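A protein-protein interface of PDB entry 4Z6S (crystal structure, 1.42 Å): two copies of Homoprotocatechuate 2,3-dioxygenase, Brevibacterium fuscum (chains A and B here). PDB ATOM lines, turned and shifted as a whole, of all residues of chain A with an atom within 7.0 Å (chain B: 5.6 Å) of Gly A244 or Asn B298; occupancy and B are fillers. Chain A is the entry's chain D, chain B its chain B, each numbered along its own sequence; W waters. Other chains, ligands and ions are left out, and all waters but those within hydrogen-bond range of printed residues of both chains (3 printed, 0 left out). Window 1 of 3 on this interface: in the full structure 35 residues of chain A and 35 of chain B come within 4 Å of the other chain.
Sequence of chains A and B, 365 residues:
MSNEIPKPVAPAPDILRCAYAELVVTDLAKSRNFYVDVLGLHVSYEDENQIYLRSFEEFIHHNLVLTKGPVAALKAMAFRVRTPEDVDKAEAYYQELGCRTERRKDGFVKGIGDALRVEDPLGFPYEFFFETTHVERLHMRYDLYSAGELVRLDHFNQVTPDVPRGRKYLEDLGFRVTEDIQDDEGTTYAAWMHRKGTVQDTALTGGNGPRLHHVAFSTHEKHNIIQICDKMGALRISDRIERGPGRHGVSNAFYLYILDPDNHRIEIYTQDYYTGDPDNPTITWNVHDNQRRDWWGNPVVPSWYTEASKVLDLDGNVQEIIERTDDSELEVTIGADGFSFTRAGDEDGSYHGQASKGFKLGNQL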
ATOM      1  N   CYS A 229       0.188  17.688 -28.640  1.00  0.00           N
ATOM      2  CA  CYS A 229      -0.711  18.634 -29.299  1.00  0.00           C
ATOM      3  C   CYS A 229      -1.511  17.942 -30.412  1.00  0.00           C
ATOM      4  O   CYS A 229      -2.731  18.132 -30.544  1.00  0.00           O
ATOM      5  CB  CYS A 229       0.076  19.785 -29.948  1.00  0.00           C
ATOM      6  SG  CYS A 229       1.057  20.784 -28.825  1.00  0.00           S
ATOM      7  N   SER A 238      -8.548  20.288 -28.393  1.00  0.00           N
ATOM      8  CA  SER A 238      -7.578  21.368 -28.578  1.00  0.00           C
ATOM      9  C   SER A 238      -7.887  22.612 -27.726  1.00  0.00           C
ATOM     10  O   SER A 238      -7.022  23.421 -27.497  1.00  0.00           O
ATOM     11  CB  SER A 238      -7.486  21.747 -30.059  1.00  0.00           C
ATOM     12  OG  SER A 238      -8.722  22.247 -30.557  1.00  0.00           O
ATOM     13  N   ILE A 241      -5.551  22.863 -24.865  1.00  0.00           N
ATOM     14  CA  ILE A 241      -4.188  23.385 -25.087  1.00  0.00           C
ATOM     15  C   ILE A 241      -4.276  24.862 -24.779  1.00  0.00           C
ATOM     16  O   ILE A 241      -4.941  25.605 -25.501  1.00  0.00           O
ATOM     17  CB  ILE A 241      -3.727  23.176 -26.541  1.00  0.00           C
ATOM     18  CG1 ILE A 241      -3.661  21.682 -26.863  1.00  0.00           C
ATOM     19  CG2 ILE A 241      -2.365  23.853 -26.778  1.00  0.00           C
ATOM     20  CD1 ILE A 241      -3.412  21.389 -28.330  1.00  0.00           C
ATOM     21  N   GLU A 242      -3.645  25.270 -23.688  1.00  0.00           N
ATOM     22  CA  GLU A 242      -3.707  26.666 -23.255  1.00  0.00           C
ATOM     23  C   GLU A 242      -2.703  27.571 -23.959  1.00  0.00           C
ATOM     24  O   GLU A 242      -3.048  28.663 -24.403  1.00  0.00           O
ATOM     25  CB  GLU A 242      -3.457  26.739 -21.747  1.00  0.00           C
ATOM     26  CG  GLU A 242      -3.754  28.131 -21.209  1.00  0.00           C
ATOM     27  CD  GLU A 242      -3.149  28.416 -19.857  1.00  0.00           C
ATOM     28  OE1 GLU A 242      -2.095  27.812 -19.518  1.00  0.00           O
ATOM     29  OE2 GLU A 242      -3.757  29.260 -19.138  1.00  0.00           O
ATOM     30  N   ARG A 243      -1.459  27.115 -24.032  1.00  0.00           N
ATOM     31  CA  ARG A 243      -0.357  27.978 -24.462  1.00  0.00           C
ATOM     32  C   ARG A 243       0.748  27.126 -25.044  1.00  0.00           C
ATOM     33  O   ARG A 243       1.155  26.158 -24.441  1.00  0.00           O
ATOM     34  CB  ARG A 243       0.197  28.808 -23.295  1.00  0.00           C
ATOM     35  CG  ARG A 243       1.406  29.631 -23.656  1.00  0.00           C
ATOM     36  CD  ARG A 243       1.985  30.483 -22.539  1.00  0.00           C
ATOM     37  NE  ARG A 243       3.313  30.917 -22.962  1.00  0.00           N
ATOM     38  CZ  ARG A 243       4.379  31.088 -22.184  1.00  0.00           C
ATOM     39  NH1 ARG A 243       4.289  30.994 -20.859  1.00  0.00           N
ATOM     40  NH2 ARG A 243       5.554  31.344 -22.747  1.00  0.00           N
ATOM     41  N   GLY A 244       1.224  27.501 -26.230  1.00  0.00           N
ATOM     42  CA  GLY A 244       2.322  26.816 -26.884  1.00  0.00           C
ATOM     43  C   GLY A 244       1.851  25.969 -28.048  1.00  0.00           C
ATOM     44  O   GLY A 244       0.738  26.163 -28.550  1.00  0.00           O
ATOM     45  N   PRO A 245       2.709  25.056 -28.522  1.00  0.00           N
ATOM     46  CA  PRO A 245       4.060  24.812 -28.067  1.00  0.00           C
ATOM     47  C   PRO A 245       5.000  25.948 -28.438  1.00  0.00           C
ATOM     48  O   PRO A 245       4.743  26.741 -29.358  1.00  0.00           O
ATOM     49  CB  PRO A 245       4.451  23.517 -28.810  1.00  0.00           C
ATOM     50  CG  PRO A 245       3.731  23.627 -30.107  1.00  0.00           C
ATOM     51  CD  PRO A 245       2.410  24.267 -29.737  1.00  0.00           C
ATOM     52  N   GLY A 246       6.084  26.054 -27.695  1.00  0.00           N
ATOM     53  CA  GLY A 246       7.079  27.067 -27.952  1.00  0.00           C
ATOM     54  C   GLY A 246       8.445  26.720 -27.449  1.00  0.00           C
ATOM     55  O   GLY A 246       8.692  25.643 -26.931  1.00  0.00           O
ATOM     56  N   TYR A 255       8.424  23.782 -24.796  1.00  0.00           N
ATOM     57  CA  TYR A 255       7.341  23.724 -23.796  1.00  0.00           C
ATOM     58  C   TYR A 255       5.947  23.650 -24.411  1.00  0.00           C
ATOM     59  O   TYR A 255       5.722  24.009 -25.575  1.00  0.00           O
ATOM     60  CB  TYR A 255       7.387  24.928 -22.864  1.00  0.00           C
ATOM     61  CG  TYR A 255       6.947  26.213 -23.518  1.00  0.00           C
ATOM     62  CD1 TYR A 255       5.618  26.598 -23.501  1.00  0.00           C
ATOM     63  CD2 TYR A 255       7.848  27.059 -24.164  1.00  0.00           C
ATOM     64  CE1 TYR A 255       5.199  27.755 -24.124  1.00  0.00           C
ATOM     65  CE2 TYR A 255       7.421  28.256 -24.754  1.00  0.00           C
ATOM     66  CZ  TYR A 255       6.102  28.606 -24.710  1.00  0.00           C
ATOM     67  OH  TYR A 255       5.637  29.778 -25.298  1.00  0.00           O
ATOM     68  N   LEU A 256       4.999  23.277 -23.552  1.00  0.00           N
ATOM     69  CA  LEU A 256       3.574  23.261 -23.875  1.00  0.00           C
ATOM     70  C   LEU A 256       2.812  23.343 -22.535  1.00  0.00           C
ATOM     71  O   LEU A 256       3.230  22.701 -21.565  1.00  0.00           O
ATOM     72  CB  LEU A 256       3.199  21.970 -24.572  1.00  0.00           C
ATOM     73  CG  LEU A 256       1.712  21.739 -24.832  1.00  0.00           C
ATOM     74  CD1 LEU A 256       1.185  22.727 -25.862  1.00  0.00           C
ATOM     75  CD2 LEU A 256       1.531  20.308 -25.288  1.00  0.00           C
ATOM     76  N   TYR A 257       1.736  24.131 -22.466  1.00  0.00           N
ATOM     77  CA  TYR A 257       0.844  24.104 -21.313  1.00  0.00           C
ATOM     78  C   TYR A 257      -0.539  23.621 -21.717  1.00  0.00           C
ATOM     79  O   TYR A 257      -1.129  24.119 -22.675  1.00  0.00           O
ATOM     80  CB  TYR A 257       0.709  25.479 -20.684  1.00  0.00           C
ATOM     81  CG  TYR A 257       2.014  26.072 -20.211  1.00  0.00           C
ATOM     82  CD1 TYR A 257       2.505  25.825 -18.908  1.00  0.00           C
ATOM     83  CD2 TYR A 257       2.808  26.838 -21.085  1.00  0.00           C
ATOM     84  CE1 TYR A 257       3.713  26.371 -18.485  1.00  0.00           C
ATOM     85  CE2 TYR A 257       4.016  27.360 -20.656  1.00  0.00           C
ATOM     86  CZ  TYR A 257       4.458  27.120 -19.371  1.00  0.00           C
ATOM     87  OH  TYR A 257       5.643  27.659 -19.001  1.00  0.00           O
ATOM     88  N   ASP A 294       8.300  33.432 -24.550  1.00  0.00           N
ATOM     89  CA  ASP A 294       8.363  32.689 -25.813  1.00  0.00           C
ATOM     90  C   ASP A 294       9.441  33.351 -26.673  1.00  0.00           C
ATOM     91  O   ASP A 294       9.345  34.518 -27.050  1.00  0.00           O
ATOM     92  CB  ASP A 294       7.028  32.745 -26.545  1.00  0.00           C
ATOM     93  CG  ASP A 294       7.005  31.767 -27.721  1.00  0.00           C
ATOM     94  OD1 ASP A 294       6.819  30.529 -27.508  1.00  0.00           O
ATOM     95  OD2 ASP A 294       7.309  32.230 -28.830  1.00  0.00           O
ATOM     96  N   ASN A 298       5.913  34.688 -29.706  1.00  0.00           N
ATOM     97  CA  ASN A 298       4.483  34.437 -29.663  1.00  0.00           C
ATOM     98  C   ASN A 298       3.865  34.979 -28.367  1.00  0.00           C
ATOM     99  O   ASN A 298       4.526  35.035 -27.334  1.00  0.00           O
ATOM    100  CB  ASN A 298       4.171  32.968 -29.878  1.00  0.00           C
ATOM    101  CG  ASN A 298       4.218  32.555 -31.324  1.00  0.00           C
ATOM    102  OD1 ASN A 298       3.833  33.313 -32.235  1.00  0.00           O
ATOM    103  ND2 ASN A 298       4.615  31.307 -31.547  1.00  0.00           N
ATOM    104  N   PRO A 299       2.606  35.424 -28.438  1.00  0.00           N
ATOM    105  CA  PRO A 299       2.034  36.129 -27.318  1.00  0.00           C
ATOM    106  C   PRO A 299       1.766  35.169 -26.180  1.00  0.00           C
ATOM    107  O   PRO A 299       1.414  34.019 -26.406  1.00  0.00           O
ATOM    108  CB  PRO A 299       0.748  36.752 -27.912  1.00  0.00           C
ATOM    109  CG  PRO A 299       0.384  35.820 -29.019  1.00  0.00           C
ATOM    110  CD  PRO A 299       1.710  35.426 -29.605  1.00  0.00           C
ATOM    111  N   VAL A 301      -0.683  33.949 -23.561  1.00  0.00           N
ATOM    112  CA  VAL A 301      -2.132  33.963 -23.466  1.00  0.00           C
ATOM    113  C   VAL A 301      -2.551  34.528 -22.081  1.00  0.00           C
ATOM    114  O   VAL A 301      -1.945  34.205 -21.059  1.00  0.00           O
ATOM    115  CB  VAL A 301      -2.720  32.565 -23.700  1.00  0.00           C
ATOM    116  CG1 VAL A 301      -2.283  31.956 -25.042  1.00  0.00           C
ATOM    117  CG2 VAL A 301      -2.415  31.626 -22.579  1.00  0.00           C
ATOM    118  N   PHE A 359      -2.544  40.534 -32.082  1.00  0.00           N
ATOM    119  CA  PHE A 359      -3.662  40.276 -31.160  1.00  0.00           C
ATOM    120  C   PHE A 359      -3.718  41.290 -30.031  1.00  0.00           C
ATOM    121  O   PHE A 359      -2.686  41.793 -29.595  1.00  0.00           O
ATOM    122  CB  PHE A 359      -3.518  38.879 -30.555  1.00  0.00           C
ATOM    123  CG  PHE A 359      -3.584  37.769 -31.571  1.00  0.00           C
ATOM    124  CD1 PHE A 359      -4.756  37.546 -32.275  1.00  0.00           C
ATOM    125  CD2 PHE A 359      -2.478  36.960 -31.807  1.00  0.00           C
ATOM    126  CE1 PHE A 359      -4.837  36.530 -33.213  1.00  0.00           C
ATOM    127  CE2 PHE A 359      -2.538  35.949 -32.755  1.00  0.00           C
ATOM    128  CZ  PHE A 359      -3.729  35.730 -33.456  1.00  0.00           C
ATOM    129  N   PRO B 245       5.172  28.225 -35.059  1.00  0.00           N
ATOM    130  CA  PRO B 245       4.922  27.022 -35.834  1.00  0.00           C
ATOM    131  C   PRO B 245       3.660  26.306 -35.389  1.00  0.00           C
ATOM    132  O   PRO B 245       3.180  26.530 -34.276  1.00  0.00           O
ATOM    133  CB  PRO B 245       6.163  26.182 -35.564  1.00  0.00           C
ATOM    134  CG  PRO B 245       6.556  26.559 -34.179  1.00  0.00           C
ATOM    135  CD  PRO B 245       6.242  28.015 -34.069  1.00  0.00           C
ATOM    136  N   ASN B 290     -12.335  25.373 -35.743  1.00  0.00           N
ATOM    137  CA  ASN B 290     -11.107  26.017 -35.271  1.00  0.00           C
ATOM    138  C   ASN B 290      -9.857  25.125 -35.340  1.00  0.00           C
ATOM    139  O   ASN B 290      -8.770  25.585 -34.958  1.00  0.00           O
ATOM    140  CB  ASN B 290     -11.287  26.477 -33.813  1.00  0.00           C
ATOM    141  CG  ASN B 290     -10.168  27.410 -33.358  1.00  0.00           C
ATOM    142  OD1 ASN B 290      -9.903  28.414 -34.006  1.00  0.00           O
ATOM    143  ND2 ASN B 290      -9.549  27.107 -32.222  1.00  0.00           N
ATOM    144  N   ASP B 294      -4.999  25.719 -37.979  1.00  0.00           N
ATOM    145  CA  ASP B 294      -4.091  25.235 -36.956  1.00  0.00           C
ATOM    146  C   ASP B 294      -4.840  24.148 -36.171  1.00  0.00           C
ATOM    147  O   ASP B 294      -5.834  24.416 -35.503  1.00  0.00           O
ATOM    148  CB  ASP B 294      -3.605  26.331 -36.029  1.00  0.00           C
ATOM    149  CG  ASP B 294      -2.506  25.828 -35.126  1.00  0.00           C
ATOM    150  OD1 ASP B 294      -1.347  25.804 -35.588  1.00  0.00           O
ATOM    151  OD2 ASP B 294      -2.811  25.383 -33.986  1.00  0.00           O
ATOM    152  N   TRP B 296      -4.107  22.558 -33.578  1.00  0.00           N
ATOM    153  CA  TRP B 296      -4.050  22.717 -32.138  1.00  0.00           C
ATOM    154  C   TRP B 296      -4.950  23.856 -31.657  1.00  0.00           C
ATOM    155  O   TRP B 296      -5.023  24.150 -30.465  1.00  0.00           O
ATOM    156  CB  TRP B 296      -2.608  22.964 -31.720  1.00  0.00           C
ATOM    157  CG  TRP B 296      -1.645  21.982 -32.256  1.00  0.00           C
ATOM    158  CD1 TRP B 296      -1.889  20.677 -32.615  1.00  0.00           C
ATOM    159  CD2 TRP B 296      -0.277  22.221 -32.553  1.00  0.00           C
ATOM    160  NE1 TRP B 296      -0.745  20.091 -33.081  1.00  0.00           N
ATOM    161  CE2 TRP B 296       0.268  21.013 -33.035  1.00  0.00           C
ATOM    162  CE3 TRP B 296       0.541  23.342 -32.443  1.00  0.00           C
ATOM    163  CZ2 TRP B 296       1.602  20.904 -33.434  1.00  0.00           C
ATOM    164  CZ3 TRP B 296       1.855  23.229 -32.797  1.00  0.00           C
ATOM    165  CH2 TRP B 296       2.380  22.023 -33.278  1.00  0.00           C
ATOM    166  N   GLY B 297      -5.670  24.476 -32.587  1.00  0.00           N
ATOM    167  CA  GLY B 297      -6.585  25.545 -32.268  1.00  0.00           C
ATOM    168  C   GLY B 297      -5.992  26.908 -32.056  1.00  0.00           C
ATOM    169  O   GLY B 297      -6.710  27.811 -31.662  1.00  0.00           O
ATOM    170  N   ASN B 298      -4.682  27.081 -32.323  1.00  0.00           N
ATOM    171  CA  ASN B 298      -4.081  28.397 -32.141  1.00  0.00           C
ATOM    172  C   ASN B 298      -4.688  29.373 -33.128  1.00  0.00           C
ATOM    173  O   ASN B 298      -5.090  28.977 -34.211  1.00  0.00           O
ATOM    174  CB  ASN B 298      -2.557  28.328 -32.253  1.00  0.00           C
ATOM    175  CG  ASN B 298      -1.916  27.825 -30.982  1.00  0.00           C
ATOM    176  OD1 ASN B 298      -2.419  28.107 -29.879  1.00  0.00           O
ATOM    177  ND2 ASN B 298      -0.800  27.093 -31.114  1.00  0.00           N
ATOM    178  N   PRO B 299      -4.781  30.652 -32.747  1.00  0.00           N
ATOM    179  CA  PRO B 299      -5.527  31.589 -33.565  1.00  0.00           C
ATOM    180  C   PRO B 299      -4.740  31.941 -34.821  1.00  0.00           C
ATOM    181  O   PRO B 299      -3.514  31.968 -34.797  1.00  0.00           O
ATOM    182  CB  PRO B 299      -5.707  32.792 -32.643  1.00  0.00           C
ATOM    183  CG  PRO B 299      -4.551  32.727 -31.708  1.00  0.00           C
ATOM    184  CD  PRO B 299      -4.354  31.246 -31.467  1.00  0.00           C
ATOM    185  N   VAL B 300      -5.433  32.160 -35.928  1.00  0.00           N
ATOM    186  CA  VAL B 300      -4.782  32.636 -37.163  1.00  0.00           C
ATOM    187  C   VAL B 300      -4.582  34.136 -37.052  1.00  0.00           C
ATOM    188  O   VAL B 300      -5.535  34.923 -36.841  1.00  0.00           O
ATOM    189  CB  VAL B 300      -5.608  32.265 -38.416  1.00  0.00           C
ATOM    190  CG1 VAL B 300      -4.922  32.743 -39.675  1.00  0.00           C
ATOM    191  CG2 VAL B 300      -5.805  30.759 -38.491  1.00  0.00           C
ATOM    192  N   SER B 356      -9.473  32.343 -30.788  1.00  0.00           N
ATOM    193  CA  SER B 356      -9.166  31.347 -29.772  1.00  0.00           C
ATOM    194  C   SER B 356      -8.063  31.815 -28.814  1.00  0.00           C
ATOM    195  O   SER B 356      -7.397  32.829 -29.050  1.00  0.00           O
ATOM    196  CB  SER B 356      -8.772  30.035 -30.460  1.00  0.00           C
ATOM    197  OG  SER B 356      -7.594  30.272 -31.237  1.00  0.00           O
ATOM    198  N   LYS B 357      -7.931  31.060 -27.723  1.00  0.00           N
ATOM    199  CA  LYS B 357      -6.866  31.145 -26.714  1.00  0.00           C
ATOM    200  C   LYS B 357      -6.847  32.468 -25.937  1.00  0.00           C
ATOM    201  O   LYS B 357      -5.856  32.804 -25.283  1.00  0.00           O
ATOM    202  CB  LYS B 357      -5.463  30.862 -27.302  1.00  0.00           C
ATOM    203  CG  LYS B 357      -5.356  29.664 -28.235  1.00  0.00           C
ATOM    204  CD  LYS B 357      -5.444  28.300 -27.549  1.00  0.00           C
ATOM    205  CE  LYS B 357      -5.244  27.159 -28.534  1.00  0.00           C
ATOM    206  NZ  LYS B 357      -5.957  25.933 -28.127  1.00  0.00           N
HETATM  207  O   HOH W   1      -0.611  29.220 -27.882  1.00  0.00           O
HETATM  208  O   HOH W   2      -9.968  24.691 -30.597  1.00  0.00           O
HETATM  209  O   HOH W   3       3.273  27.632 -31.653  1.00  0.00           O
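Water W2 lies within hydrogen-bond range of the side-chain hydroxyl of Ser A238 (2.7 Å) and the side-chain amide nitrogen of Asn B290 (2.9 Å). Water W3 lies within hydrogen-bond range of the backbone carbonyl oxygen of Pro B245 (2.8 Å) and the backbone carbonyl oxygen of Pro A245 (2.9 Å). Water W1 lies within hydrogen-bond range of the side-chain amide oxygen of Asn B298 (2.9 Å) and the backbone NH of Gly A244 (3.0 Å).
ND2 of Asn B298 sits at hydrogen-bond distance from O of Gly A244 (3.1 Å). NZ of Lys B357 lies within hydrogen-bond range of O of Ser A238. NZ of Lys B357 lies within hydrogen-bond range of O of Ile A241, at 2.8 Å.
Trp B296 touches Cys A229. Trp B296 touches Ser A238. CB of Trp B296 touches CD1 of Ile A241 (3.8 Å). O of Glu A242 touches CD of Lys B357, 3.97 Å away. CD of Pro A245 touches CZ3 of Trp B296, 3.3 Å away. CB of Val A301 touches O of Lys B357 (3.5 Å). Pro B299 touches Phe A359. Val B300 touches Phe A359 (O to CZ, 3.9 Å).
The backbone NH (N) of Trp B296 lies close to the side-chain carboxylate (OD2) of Asp B294 (3.1 Å). The side-chain carboxylate (OD2) of Asp B294 lies within hydrogen-bond range of the backbone NH (N) of Asn B298 (3.0 Å). The side-chain amino group (NZ) of Lys B357 sits at hydrogen-bond distance from the backbone carbonyl oxygen (O) of Trp B296, at 3.1 Å. The backbone carbonyl oxygen (O) of Tyr A257 is in hydrogen-bond range of the backbone NH (N) of Glu A242 (2.9 Å).
Of the printed residues of chain B, Ser A238 touches Trp B296 (3.5 Å) and Lys B357 (2.8 Å). Of the printed residues of chain B, Ile A241 touches Trp B296 (3.8 Å) and Lys B357 (2.8 Å). Printed residues of chain B within 4 Å of Glu A242: Lys B357. Printed residues of chain B within 4 Å of Gly A244: Asn B298. Asn A298 touches none of the printed residues of chain B. Pro B245 touches none of the printed residues of chain A. Of the printed residues of chain A, Trp B296 touches Cys A229, Ser A238, Ile A241 and Pro A245. Of chain A, only Gly A244 comes within 4 Å of Asn B298. Of the printed residues of chain A, Lys B357 touches Ser A238, Ile A241, Glu A242 and Val A301. The nearest residue of chain A that does not touch Asn B298 is Pro A245 (4.5 Å). The nearest printed residue of chain A that does not touch Pro B299 is Pro A299 (6.4 Å).
Of the 16 printed residues of chain A, 8 touch a printed residue of chain B. Hydrophobic or aromatic side chains of chain A within 4 Å of the printed part of chain B: Ile A241, Pro A245, Val A301 and Phe A359. Hydrophobic or aromatic side chains of chain B within 4 Å of the printed part of chain A: Trp B296 and Pro B299. Among the printed residues, 11 pairs touch across the chains.
4 positions are printed for both chains. Of the 11 pairs that touch across the chains among the printed residues, none has its exchanged pair printed and touching as well.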
